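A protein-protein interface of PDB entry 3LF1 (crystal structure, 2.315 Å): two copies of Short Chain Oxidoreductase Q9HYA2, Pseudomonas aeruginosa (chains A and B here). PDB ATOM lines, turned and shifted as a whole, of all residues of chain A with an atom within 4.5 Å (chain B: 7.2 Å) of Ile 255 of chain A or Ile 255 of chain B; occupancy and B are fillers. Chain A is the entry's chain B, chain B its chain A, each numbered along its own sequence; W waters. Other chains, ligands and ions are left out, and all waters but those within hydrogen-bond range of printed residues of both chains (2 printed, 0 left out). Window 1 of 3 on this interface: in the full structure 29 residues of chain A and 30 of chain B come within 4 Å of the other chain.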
ATOM      1  N   GLY A 186       6.077 -18.960 -37.394  1.00  0.00           N
ATOM      2  CA  GLY A 186       5.028 -18.059 -37.802  1.00  0.00           C
ATOM      3  C   GLY A 186       4.809 -16.946 -36.798  1.00  0.00           C
ATOM      4  O   GLY A 186       5.482 -16.865 -35.774  1.00  0.00           O
ATOM      5  N   ILE A 187       3.854 -16.077 -37.094  1.00  0.00           N
ATOM      6  CA  ILE A 187       3.456 -15.072 -36.121  1.00  0.00           C
ATOM      7  C   ILE A 187       1.941 -15.077 -35.981  1.00  0.00           C
ATOM      8  O   ILE A 187       1.237 -15.649 -36.818  1.00  0.00           O
ATOM      9  CB  ILE A 187       4.002 -13.655 -36.479  1.00  0.00           C
ATOM     10  CG1 ILE A 187       3.226 -13.034 -37.626  1.00  0.00           C
ATOM     11  CG2 ILE A 187       5.492 -13.727 -36.804  1.00  0.00           C
ATOM     12  CD1 ILE A 187       3.400 -11.533 -37.717  1.00  0.00           C
ATOM     13  N   LEU A 188       1.439 -14.466 -34.916  1.00  0.00           N
ATOM     14  CA  LEU A 188       0.005 -14.416 -34.717  1.00  0.00           C
ATOM     15  C   LEU A 188      -0.399 -12.969 -34.534  1.00  0.00           C
ATOM     16  O   LEU A 188      -0.310 -12.419 -33.438  1.00  0.00           O
ATOM     17  CB  LEU A 188      -0.412 -15.271 -33.515  1.00  0.00           C
ATOM     18  CG  LEU A 188      -0.073 -16.767 -33.642  1.00  0.00           C
ATOM     19  CD1 LEU A 188      -0.342 -17.531 -32.351  1.00  0.00           C
ATOM     20  CD2 LEU A 188      -0.808 -17.418 -34.839  1.00  0.00           C
ATOM     21  N   ALA A 238       8.770  -8.753 -36.439  1.00  0.00           N
ATOM     22  CA  ALA A 238       8.739 -10.073 -35.841  1.00  0.00           C
ATOM     23  C   ALA A 238       9.040 -11.108 -36.915  1.00  0.00           C
ATOM     24  O   ALA A 238       9.717 -12.108 -36.667  1.00  0.00           O
ATOM     25  CB  ALA A 238       7.379 -10.338 -35.194  1.00  0.00           C
ATOM     26  N   PHE A 241      12.662 -10.905 -37.426  1.00  0.00           N
ATOM     27  CA  PHE A 241      13.361 -11.603 -36.363  1.00  0.00           C
ATOM     28  C   PHE A 241      13.428 -13.119 -36.664  1.00  0.00           C
ATOM     29  O   PHE A 241      14.513 -13.713 -36.687  1.00  0.00           O
ATOM     30  CB  PHE A 241      12.714 -11.336 -35.009  1.00  0.00           C
ATOM     31  CG  PHE A 241      13.327 -12.134 -33.894  1.00  0.00           C
ATOM     32  CD1 PHE A 241      14.525 -11.711 -33.293  1.00  0.00           C
ATOM     33  CD2 PHE A 241      12.728 -13.299 -33.451  1.00  0.00           C
ATOM     34  CE1 PHE A 241      15.114 -12.445 -32.272  1.00  0.00           C
ATOM     35  CE2 PHE A 241      13.299 -14.042 -32.421  1.00  0.00           C
ATOM     36  CZ  PHE A 241      14.497 -13.625 -31.836  1.00  0.00           C
ATOM     37  N   LEU A 242      12.263 -13.709 -36.938  1.00  0.00           N
ATOM     38  CA  LEU A 242      12.112 -15.139 -37.202  1.00  0.00           C
ATOM     39  C   LEU A 242      12.776 -15.599 -38.496  1.00  0.00           C
ATOM     40  O   LEU A 242      13.218 -16.752 -38.601  1.00  0.00           O
ATOM     41  CB  LEU A 242      10.623 -15.502 -37.254  1.00  0.00           C
ATOM     42  CG  LEU A 242       9.908 -15.466 -35.903  1.00  0.00           C
ATOM     43  CD1 LEU A 242       8.424 -15.746 -36.093  1.00  0.00           C
ATOM     44  CD2 LEU A 242      10.523 -16.497 -34.955  1.00  0.00           C
ATOM     45  N   HIS A 254       5.662 -19.767 -32.684  1.00  0.00           N
ATOM     46  CA  HIS A 254       4.990 -18.556 -33.141  1.00  0.00           C
ATOM     47  C   HIS A 254       5.342 -17.377 -32.244  1.00  0.00           C
ATOM     48  O   HIS A 254       5.727 -17.554 -31.087  1.00  0.00           O
ATOM     49  CB  HIS A 254       3.470 -18.757 -33.158  1.00  0.00           C
ATOM     50  CG  HIS A 254       2.990 -19.528 -34.345  1.00  0.00           C
ATOM     51  ND1 HIS A 254       3.227 -20.879 -34.498  1.00  0.00           N
ATOM     52  CD2 HIS A 254       2.321 -19.133 -35.453  1.00  0.00           C
ATOM     53  CE1 HIS A 254       2.728 -21.278 -35.654  1.00  0.00           C
ATOM     54  NE2 HIS A 254       2.159 -20.242 -36.246  1.00  0.00           N
ATOM     55  N   ILE A 255       5.234 -16.168 -32.782  1.00  0.00           N
ATOM     56  CA  ILE A 255       5.415 -14.986 -31.962  1.00  0.00           C
ATOM     57  C   ILE A 255       4.100 -14.238 -31.941  1.00  0.00           C
ATOM     58  O   ILE A 255       3.476 -14.018 -32.984  1.00  0.00           O
ATOM     59  CB  ILE A 255       6.529 -14.049 -32.488  1.00  0.00           C
ATOM     60  CG1 ILE A 255       7.903 -14.660 -32.241  1.00  0.00           C
ATOM     61  CG2 ILE A 255       6.416 -12.663 -31.847  1.00  0.00           C
ATOM     62  CD1 ILE A 255       9.047 -13.728 -32.555  1.00  0.00           C
ATOM     63  N   ASP A 256       3.695 -13.853 -30.737  1.00  0.00           N
ATOM     64  CA  ASP A 256       2.475 -13.102 -30.519  1.00  0.00           C
ATOM     65  C   ASP A 256       2.641 -11.618 -30.907  1.00  0.00           C
ATOM     66  O   ASP A 256       3.538 -10.939 -30.424  1.00  0.00           O
ATOM     67  CB  ASP A 256       2.087 -13.248 -29.056  1.00  0.00           C
ATOM     68  CG  ASP A 256       0.722 -12.687 -28.755  1.00  0.00           C
ATOM     69  OD1 ASP A 256       0.320 -11.700 -29.415  1.00  0.00           O
ATOM     70  OD2 ASP A 256       0.065 -13.230 -27.838  1.00  0.00           O
ATOM     71  N   VAL A 257       1.782 -11.127 -31.793  1.00  0.00           N
ATOM     72  CA  VAL A 257       1.825  -9.724 -32.212  1.00  0.00           C
ATOM     73  C   VAL A 257       0.404  -9.155 -32.188  1.00  0.00           C
ATOM     74  O   VAL A 257      -0.067  -8.587 -33.173  1.00  0.00           O
ATOM     75  CB  VAL A 257       2.485  -9.533 -33.628  1.00  0.00           C
ATOM     76  CG1 VAL A 257       2.623  -8.061 -33.949  1.00  0.00           C
ATOM     77  CG2 VAL A 257       3.880 -10.202 -33.708  1.00  0.00           C
ATOM     78  N   ASN B 145      12.735 -17.925 -18.905  1.00  0.00           N
ATOM     79  CA  ASN B 145      12.059 -19.126 -18.455  1.00  0.00           C
ATOM     80  C   ASN B 145      12.513 -20.297 -19.332  1.00  0.00           C
ATOM     81  O   ASN B 145      13.306 -20.112 -20.260  1.00  0.00           O
ATOM     82  CB  ASN B 145      10.543 -18.912 -18.516  1.00  0.00           C
ATOM     83  CG  ASN B 145       9.772 -19.788 -17.518  1.00  0.00           C
ATOM     84  OD1 ASN B 145      10.207 -20.880 -17.162  1.00  0.00           O
ATOM     85  ND2 ASN B 145       8.619 -19.304 -17.076  1.00  0.00           N
ATOM     86  N   ASN B 185       7.030  -9.790 -21.283  1.00  0.00           N
ATOM     87  CA  ASN B 185       7.108 -11.048 -22.009  1.00  0.00           C
ATOM     88  C   ASN B 185       8.167 -11.936 -21.384  1.00  0.00           C
ATOM     89  O   ASN B 185       8.842 -11.536 -20.437  1.00  0.00           O
ATOM     90  CB  ASN B 185       7.428 -10.806 -23.487  1.00  0.00           C
ATOM     91  CG  ASN B 185       6.380  -9.934 -24.178  1.00  0.00           C
ATOM     92  OD1 ASN B 185       5.351 -10.424 -24.652  1.00  0.00           O
ATOM     93  ND2 ASN B 185       6.638  -8.639 -24.231  1.00  0.00           N
ATOM     94  N   GLY B 186       8.302 -13.149 -21.906  1.00  0.00           N
ATOM     95  CA  GLY B 186       9.374 -14.026 -21.491  1.00  0.00           C
ATOM     96  C   GLY B 186       9.862 -14.904 -22.635  1.00  0.00           C
ATOM     97  O   GLY B 186       9.385 -14.812 -23.775  1.00  0.00           O
ATOM     98  N   ILE B 187      10.820 -15.771 -22.329  1.00  0.00           N
ATOM     99  CA  ILE B 187      11.262 -16.738 -23.311  1.00  0.00           C
ATOM    100  C   ILE B 187      11.245 -18.144 -22.720  1.00  0.00           C
ATOM    101  O   ILE B 187      11.208 -18.318 -21.492  1.00  0.00           O
ATOM    102  CB  ILE B 187      12.651 -16.401 -23.909  1.00  0.00           C
ATOM    103  CG1 ILE B 187      13.782 -16.715 -22.923  1.00  0.00           C
ATOM    104  CG2 ILE B 187      12.697 -14.957 -24.369  1.00  0.00           C
ATOM    105  CD1 ILE B 187      15.138 -16.843 -23.625  1.00  0.00           C
ATOM    106  N   LEU B 188      11.220 -19.145 -23.600  1.00  0.00           N
ATOM    107  CA  LEU B 188      11.245 -20.537 -23.165  1.00  0.00           C
ATOM    108  C   LEU B 188      12.482 -21.216 -23.718  1.00  0.00           C
ATOM    109  O   LEU B 188      12.493 -21.677 -24.851  1.00  0.00           O
ATOM    110  CB  LEU B 188       9.970 -21.271 -23.589  1.00  0.00           C
ATOM    111  CG  LEU B 188       8.712 -20.566 -23.051  1.00  0.00           C
ATOM    112  CD1 LEU B 188       7.439 -21.122 -23.640  1.00  0.00           C
ATOM    113  CD2 LEU B 188       8.664 -20.593 -21.518  1.00  0.00           C
ATOM    114  N   ILE B 189      13.541 -21.283 -22.926  1.00  0.00           N
ATOM    115  CA  ILE B 189      14.754 -21.900 -23.440  1.00  0.00           C
ATOM    116  C   ILE B 189      14.614 -23.405 -23.433  1.00  0.00           C
ATOM    117  O   ILE B 189      13.898 -23.973 -22.611  1.00  0.00           O
ATOM    118  CB  ILE B 189      16.012 -21.513 -22.648  1.00  0.00           C
ATOM    119  CG1 ILE B 189      15.897 -21.992 -21.195  1.00  0.00           C
ATOM    120  CG2 ILE B 189      16.276 -20.002 -22.758  1.00  0.00           C
ATOM    121  CD1 ILE B 189      17.198 -21.835 -20.397  1.00  0.00           C
ATOM    122  N   ARG B 237      19.479 -13.035 -27.758  1.00  0.00           N
ATOM    123  CA  ARG B 237      18.920 -12.348 -28.920  1.00  0.00           C
ATOM    124  C   ARG B 237      17.390 -12.237 -28.875  1.00  0.00           C
ATOM    125  O   ARG B 237      16.824 -11.220 -29.284  1.00  0.00           O
ATOM    126  CB  ARG B 237      19.422 -12.984 -30.210  1.00  0.00           C
ATOM    127  CG  ARG B 237      20.751 -12.392 -30.657  1.00  0.00           C
ATOM    128  CD  ARG B 237      21.513 -13.342 -31.558  1.00  0.00           C
ATOM    129  NE  ARG B 237      22.754 -12.750 -32.040  1.00  0.00           N
ATOM    130  CZ  ARG B 237      23.835 -13.466 -32.324  1.00  0.00           C
ATOM    131  NH1 ARG B 237      24.946 -12.888 -32.764  1.00  0.00           N
ATOM    132  NH2 ARG B 237      23.804 -14.778 -32.148  1.00  0.00           N
ATOM    133  N   ALA B 238      16.731 -13.253 -28.320  1.00  0.00           N
ATOM    134  CA  ALA B 238      15.278 -13.230 -28.174  1.00  0.00           C
ATOM    135  C   ALA B 238      14.876 -12.286 -27.050  1.00  0.00           C
ATOM    136  O   ALA B 238      13.838 -11.618 -27.109  1.00  0.00           O
ATOM    137  CB  ALA B 238      14.736 -14.647 -27.912  1.00  0.00           C
ATOM    138  N   ILE B 239      15.688 -12.257 -26.006  1.00  0.00           N
ATOM    139  CA  ILE B 239      15.461 -11.333 -24.898  1.00  0.00           C
ATOM    140  C   ILE B 239      15.557  -9.858 -25.368  1.00  0.00           C
ATOM    141  O   ILE B 239      14.693  -9.036 -25.067  1.00  0.00           O
ATOM    142  CB  ILE B 239      16.444 -11.641 -23.746  1.00  0.00           C
ATOM    143  CG1 ILE B 239      16.151 -13.038 -23.182  1.00  0.00           C
ATOM    144  CG2 ILE B 239      16.373 -10.589 -22.651  1.00  0.00           C
ATOM    145  CD1 ILE B 239      17.154 -13.523 -22.157  1.00  0.00           C
ATOM    146  N   PHE B 241      15.172  -8.691 -28.496  1.00  0.00           N
ATOM    147  CA  PHE B 241      13.957  -8.450 -29.257  1.00  0.00           C
ATOM    148  C   PHE B 241      12.772  -8.031 -28.362  1.00  0.00           C
ATOM    149  O   PHE B 241      12.130  -7.009 -28.615  1.00  0.00           O
ATOM    150  CB  PHE B 241      13.594  -9.668 -30.095  1.00  0.00           C
ATOM    151  CG  PHE B 241      12.371  -9.461 -30.943  1.00  0.00           C
ATOM    152  CD1 PHE B 241      12.426  -8.649 -32.066  1.00  0.00           C
ATOM    153  CD2 PHE B 241      11.177 -10.072 -30.625  1.00  0.00           C
ATOM    154  CE1 PHE B 241      11.317  -8.448 -32.854  1.00  0.00           C
ATOM    155  CE2 PHE B 241      10.054  -9.879 -31.414  1.00  0.00           C
ATOM    156  CZ  PHE B 241      10.121  -9.063 -32.530  1.00  0.00           C
ATOM    157  N   LEU B 242      12.506  -8.797 -27.305  1.00  0.00           N
ATOM    158  CA  LEU B 242      11.391  -8.496 -26.390  1.00  0.00           C
ATOM    159  C   LEU B 242      11.576  -7.206 -25.563  1.00  0.00           C
ATOM    160  O   LEU B 242      10.620  -6.496 -25.249  1.00  0.00           O
ATOM    161  CB  LEU B 242      11.156  -9.676 -25.440  1.00  0.00           C
ATOM    162  CG  LEU B 242      10.278 -10.855 -25.921  1.00  0.00           C
ATOM    163  CD1 LEU B 242       9.236 -10.436 -26.962  1.00  0.00           C
ATOM    164  CD2 LEU B 242      11.102 -12.008 -26.426  1.00  0.00           C
ATOM    165  N   SER B 247       9.647  -4.947 -30.607  1.00  0.00           N
ATOM    166  CA  SER B 247       8.475  -5.776 -30.309  1.00  0.00           C
ATOM    167  C   SER B 247       7.363  -4.964 -29.624  1.00  0.00           C
ATOM    168  O   SER B 247       6.675  -5.454 -28.735  1.00  0.00           O
ATOM    169  CB  SER B 247       8.887  -6.969 -29.431  1.00  0.00           C
ATOM    170  OG  SER B 247       9.492  -6.536 -28.218  1.00  0.00           O
ATOM    171  N   THR B 250       3.943  -6.433 -28.699  1.00  0.00           N
ATOM    172  CA  THR B 250       3.992  -7.756 -28.102  1.00  0.00           C
ATOM    173  C   THR B 250       4.042  -7.659 -26.579  1.00  0.00           C
ATOM    174  O   THR B 250       4.972  -7.072 -26.008  1.00  0.00           O
ATOM    175  CB  THR B 250       5.227  -8.530 -28.610  1.00  0.00           C
ATOM    176  OG1 THR B 250       5.123  -8.700 -30.029  1.00  0.00           O
ATOM    177  CG2 THR B 250       5.328  -9.898 -27.942  1.00  0.00           C
ATOM    178  N   SER B 253       3.362 -12.564 -23.834  1.00  0.00           N
ATOM    179  CA  SER B 253       3.668 -13.707 -24.682  1.00  0.00           C
ATOM    180  C   SER B 253       5.038 -14.282 -24.358  1.00  0.00           C
ATOM    181  O   SER B 253       5.742 -13.776 -23.491  1.00  0.00           O
ATOM    182  CB  SER B 253       3.640 -13.306 -26.165  1.00  0.00           C
ATOM    183  OG  SER B 253       4.802 -12.559 -26.516  1.00  0.00           O
ATOM    184  N   HIS B 254       5.399 -15.360 -25.049  1.00  0.00           N
ATOM    185  CA  HIS B 254       6.696 -16.008 -24.862  1.00  0.00           C
ATOM    186  C   HIS B 254       7.297 -16.359 -26.217  1.00  0.00           C
ATOM    187  O   HIS B 254       6.585 -16.551 -27.192  1.00  0.00           O
ATOM    188  CB  HIS B 254       6.560 -17.261 -23.990  1.00  0.00           C
ATOM    189  CG  HIS B 254       6.505 -16.957 -22.524  1.00  0.00           C
ATOM    190  ND1 HIS B 254       5.376 -16.464 -21.910  1.00  0.00           N
ATOM    191  CD2 HIS B 254       7.450 -17.045 -21.560  1.00  0.00           C
ATOM    192  CE1 HIS B 254       5.623 -16.265 -20.627  1.00  0.00           C
ATOM    193  NE2 HIS B 254       6.872 -16.618 -20.388  1.00  0.00           N
ATOM    194  N   ILE B 255       8.614 -16.428 -26.277  1.00  0.00           N
ATOM    195  CA  ILE B 255       9.281 -16.812 -27.510  1.00  0.00           C
ATOM    196  C   ILE B 255       9.957 -18.122 -27.231  1.00  0.00           C
ATOM    197  O   ILE B 255      10.626 -18.273 -26.213  1.00  0.00           O
ATOM    198  CB  ILE B 255      10.318 -15.749 -27.973  1.00  0.00           C
ATOM    199  CG1 ILE B 255       9.591 -14.532 -28.537  1.00  0.00           C
ATOM    200  CG2 ILE B 255      11.315 -16.343 -28.972  1.00  0.00           C
ATOM    201  CD1 ILE B 255      10.484 -13.590 -29.304  1.00  0.00           C
ATOM    202  N   ASP B 256       9.769 -19.066 -28.139  1.00  0.00           N
ATOM    203  CA  ASP B 256      10.353 -20.388 -28.009  1.00  0.00           C
ATOM    204  C   ASP B 256      11.828 -20.343 -28.447  1.00  0.00           C
ATOM    205  O   ASP B 256      12.138 -19.925 -29.558  1.00  0.00           O
ATOM    206  CB  ASP B 256       9.551 -21.371 -28.868  1.00  0.00           C
ATOM    207  CG  ASP B 256      10.022 -22.811 -28.736  1.00  0.00           C
ATOM    208  OD1 ASP B 256      11.224 -23.058 -28.497  1.00  0.00           O
ATOM    209  OD2 ASP B 256       9.171 -23.717 -28.902  1.00  0.00           O
ATOM    210  N   VAL B 257      12.735 -20.738 -27.559  1.00  0.00           N
ATOM    211  CA  VAL B 257      14.141 -20.862 -27.911  1.00  0.00           C
ATOM    212  C   VAL B 257      14.674 -22.252 -27.519  1.00  0.00           C
ATOM    213  O   VAL B 257      15.626 -22.374 -26.749  1.00  0.00           O
ATOM    214  CB  VAL B 257      14.990 -19.734 -27.266  1.00  0.00           C
ATOM    215  CG1 VAL B 257      16.384 -19.684 -27.905  1.00  0.00           C
ATOM    216  CG2 VAL B 257      14.304 -18.393 -27.430  1.00  0.00           C
ATOM    217  N   SER B 258      14.057 -23.298 -28.058  1.00  0.00           N
ATOM    218  CA  SER B 258      14.350 -24.659 -27.601  1.00  0.00           C
ATOM    219  C   SER B 258      14.851 -25.540 -28.732  1.00  0.00           C
ATOM    220  O   SER B 258      15.083 -26.726 -28.541  1.00  0.00           O
ATOM    221  CB  SER B 258      13.107 -25.297 -26.953  1.00  0.00           C
ATOM    222  OG  SER B 258      12.073 -25.562 -27.900  1.00  0.00           O
HETATM  223  O   HOH W   1       5.603 -14.284 -28.344  1.00  0.00           O
HETATM  224  O   HOH W   2       8.366 -18.275 -30.688  1.00  0.00           O
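Water W1 lies within hydrogen-bond range of OG of Ser 253 of chain B (2.6 Å), O of His 254 of chain B (2.7 Å) and N of Asp 256 of chain A (3.1 Å). Water W2 bridges the backbone carbonyl oxygen (O) of His 254 of chain A (2.8 Å) and the backbone NH (N) of Asp 256 of chain B (3.0 Å).
Of the printed residues of chain B, Ala 238 of chain A touches Phe 241. Ile 255 of chain A touches one residue of chain B. Gly 186 of chain B touches none of the printed residues of chain A. Leu 188 of chain B touches none of the printed residues of chain A. Of the printed residues of chain A, Arg 237 of chain B touches Phe 241 (3.7 Å). Of the printed residues of chain A, Ala 238 of chain B touches Phe 241. Of chain A, only Ile 255 (3.6 Å) comes within 4 Å of Ile 255 of chain B.
Of the 19 printed residues of chain B, 6 touch a printed residue of chain A. Of the 10 printed residues of chain A, 4 touch a printed residue of chain B. Along chain A the printed residues that touch a printed residue of chain B span positions 238 to 256.
The side-chain hydroxyl (OG1) of Thr 250 of chain B lies within hydrogen-bond range of the backbone carbonyl oxygen (O) of Asp 256 of chain A (2.8 Å).
CA of Ala 238 of chain A touches CZ of Phe 241 of chain B, 3.7 Å away. Phe 241 of chain A touches Arg 237 of chain B. Ala 238 of chain B touches Phe 241 of chain A (CA to CZ, 3.8 Å). CB of Phe 241 of chain B touches CE1 of Phe 241 of chain A, 3.8 Å away. CD1 of Ile 255 of chain B touches CD1 of Ile 255 of chain A, 3.6 Å away. Asp 256 of chain A touches Ser 253 of chain B.
Ala 238 of chain A touches Phe 241 of chain B, and with the chains exchanged Phe 241 of chain A touches Ala 238 of chain B. Phe 241 of chain A touches its own counterpart, Phe 241 of chain B. Ile 255 of chain A touches its own counterpart, Ile 255 of chain B. 10 positions are printed for both chains.
The side-chain amide nitrogen (ND2) of Asn 185 of chain B is in hydrogen-bond range of the backbone carbonyl oxygen (O) of Thr 250 of chain B (2.9 Å). OD1 of Asn 185 of chain B is in hydrogen-bond range of OG of Ser 253 of chain B, at 2.9 Å. The backbone carbonyl oxygen (O) of Ile 255 of chain B is in hydrogen-bond range of the backbone NH (N) of Leu 188 of chain B (2.8 Å). OG of Ser 247 of chain B sits at hydrogen-bond distance from O of Phe 241 of chain B. The backbone carbonyl oxygen of Gly 186 of chain B lies within hydrogen-bond range of the backbone NH of Ile 255 of chain B, 3.1 Å away. The backbone NH (N) of Leu 188 of chain A sits at hydrogen-bond distance from the backbone carbonyl oxygen (O) of Ile 255 of chain A (2.8 Å).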
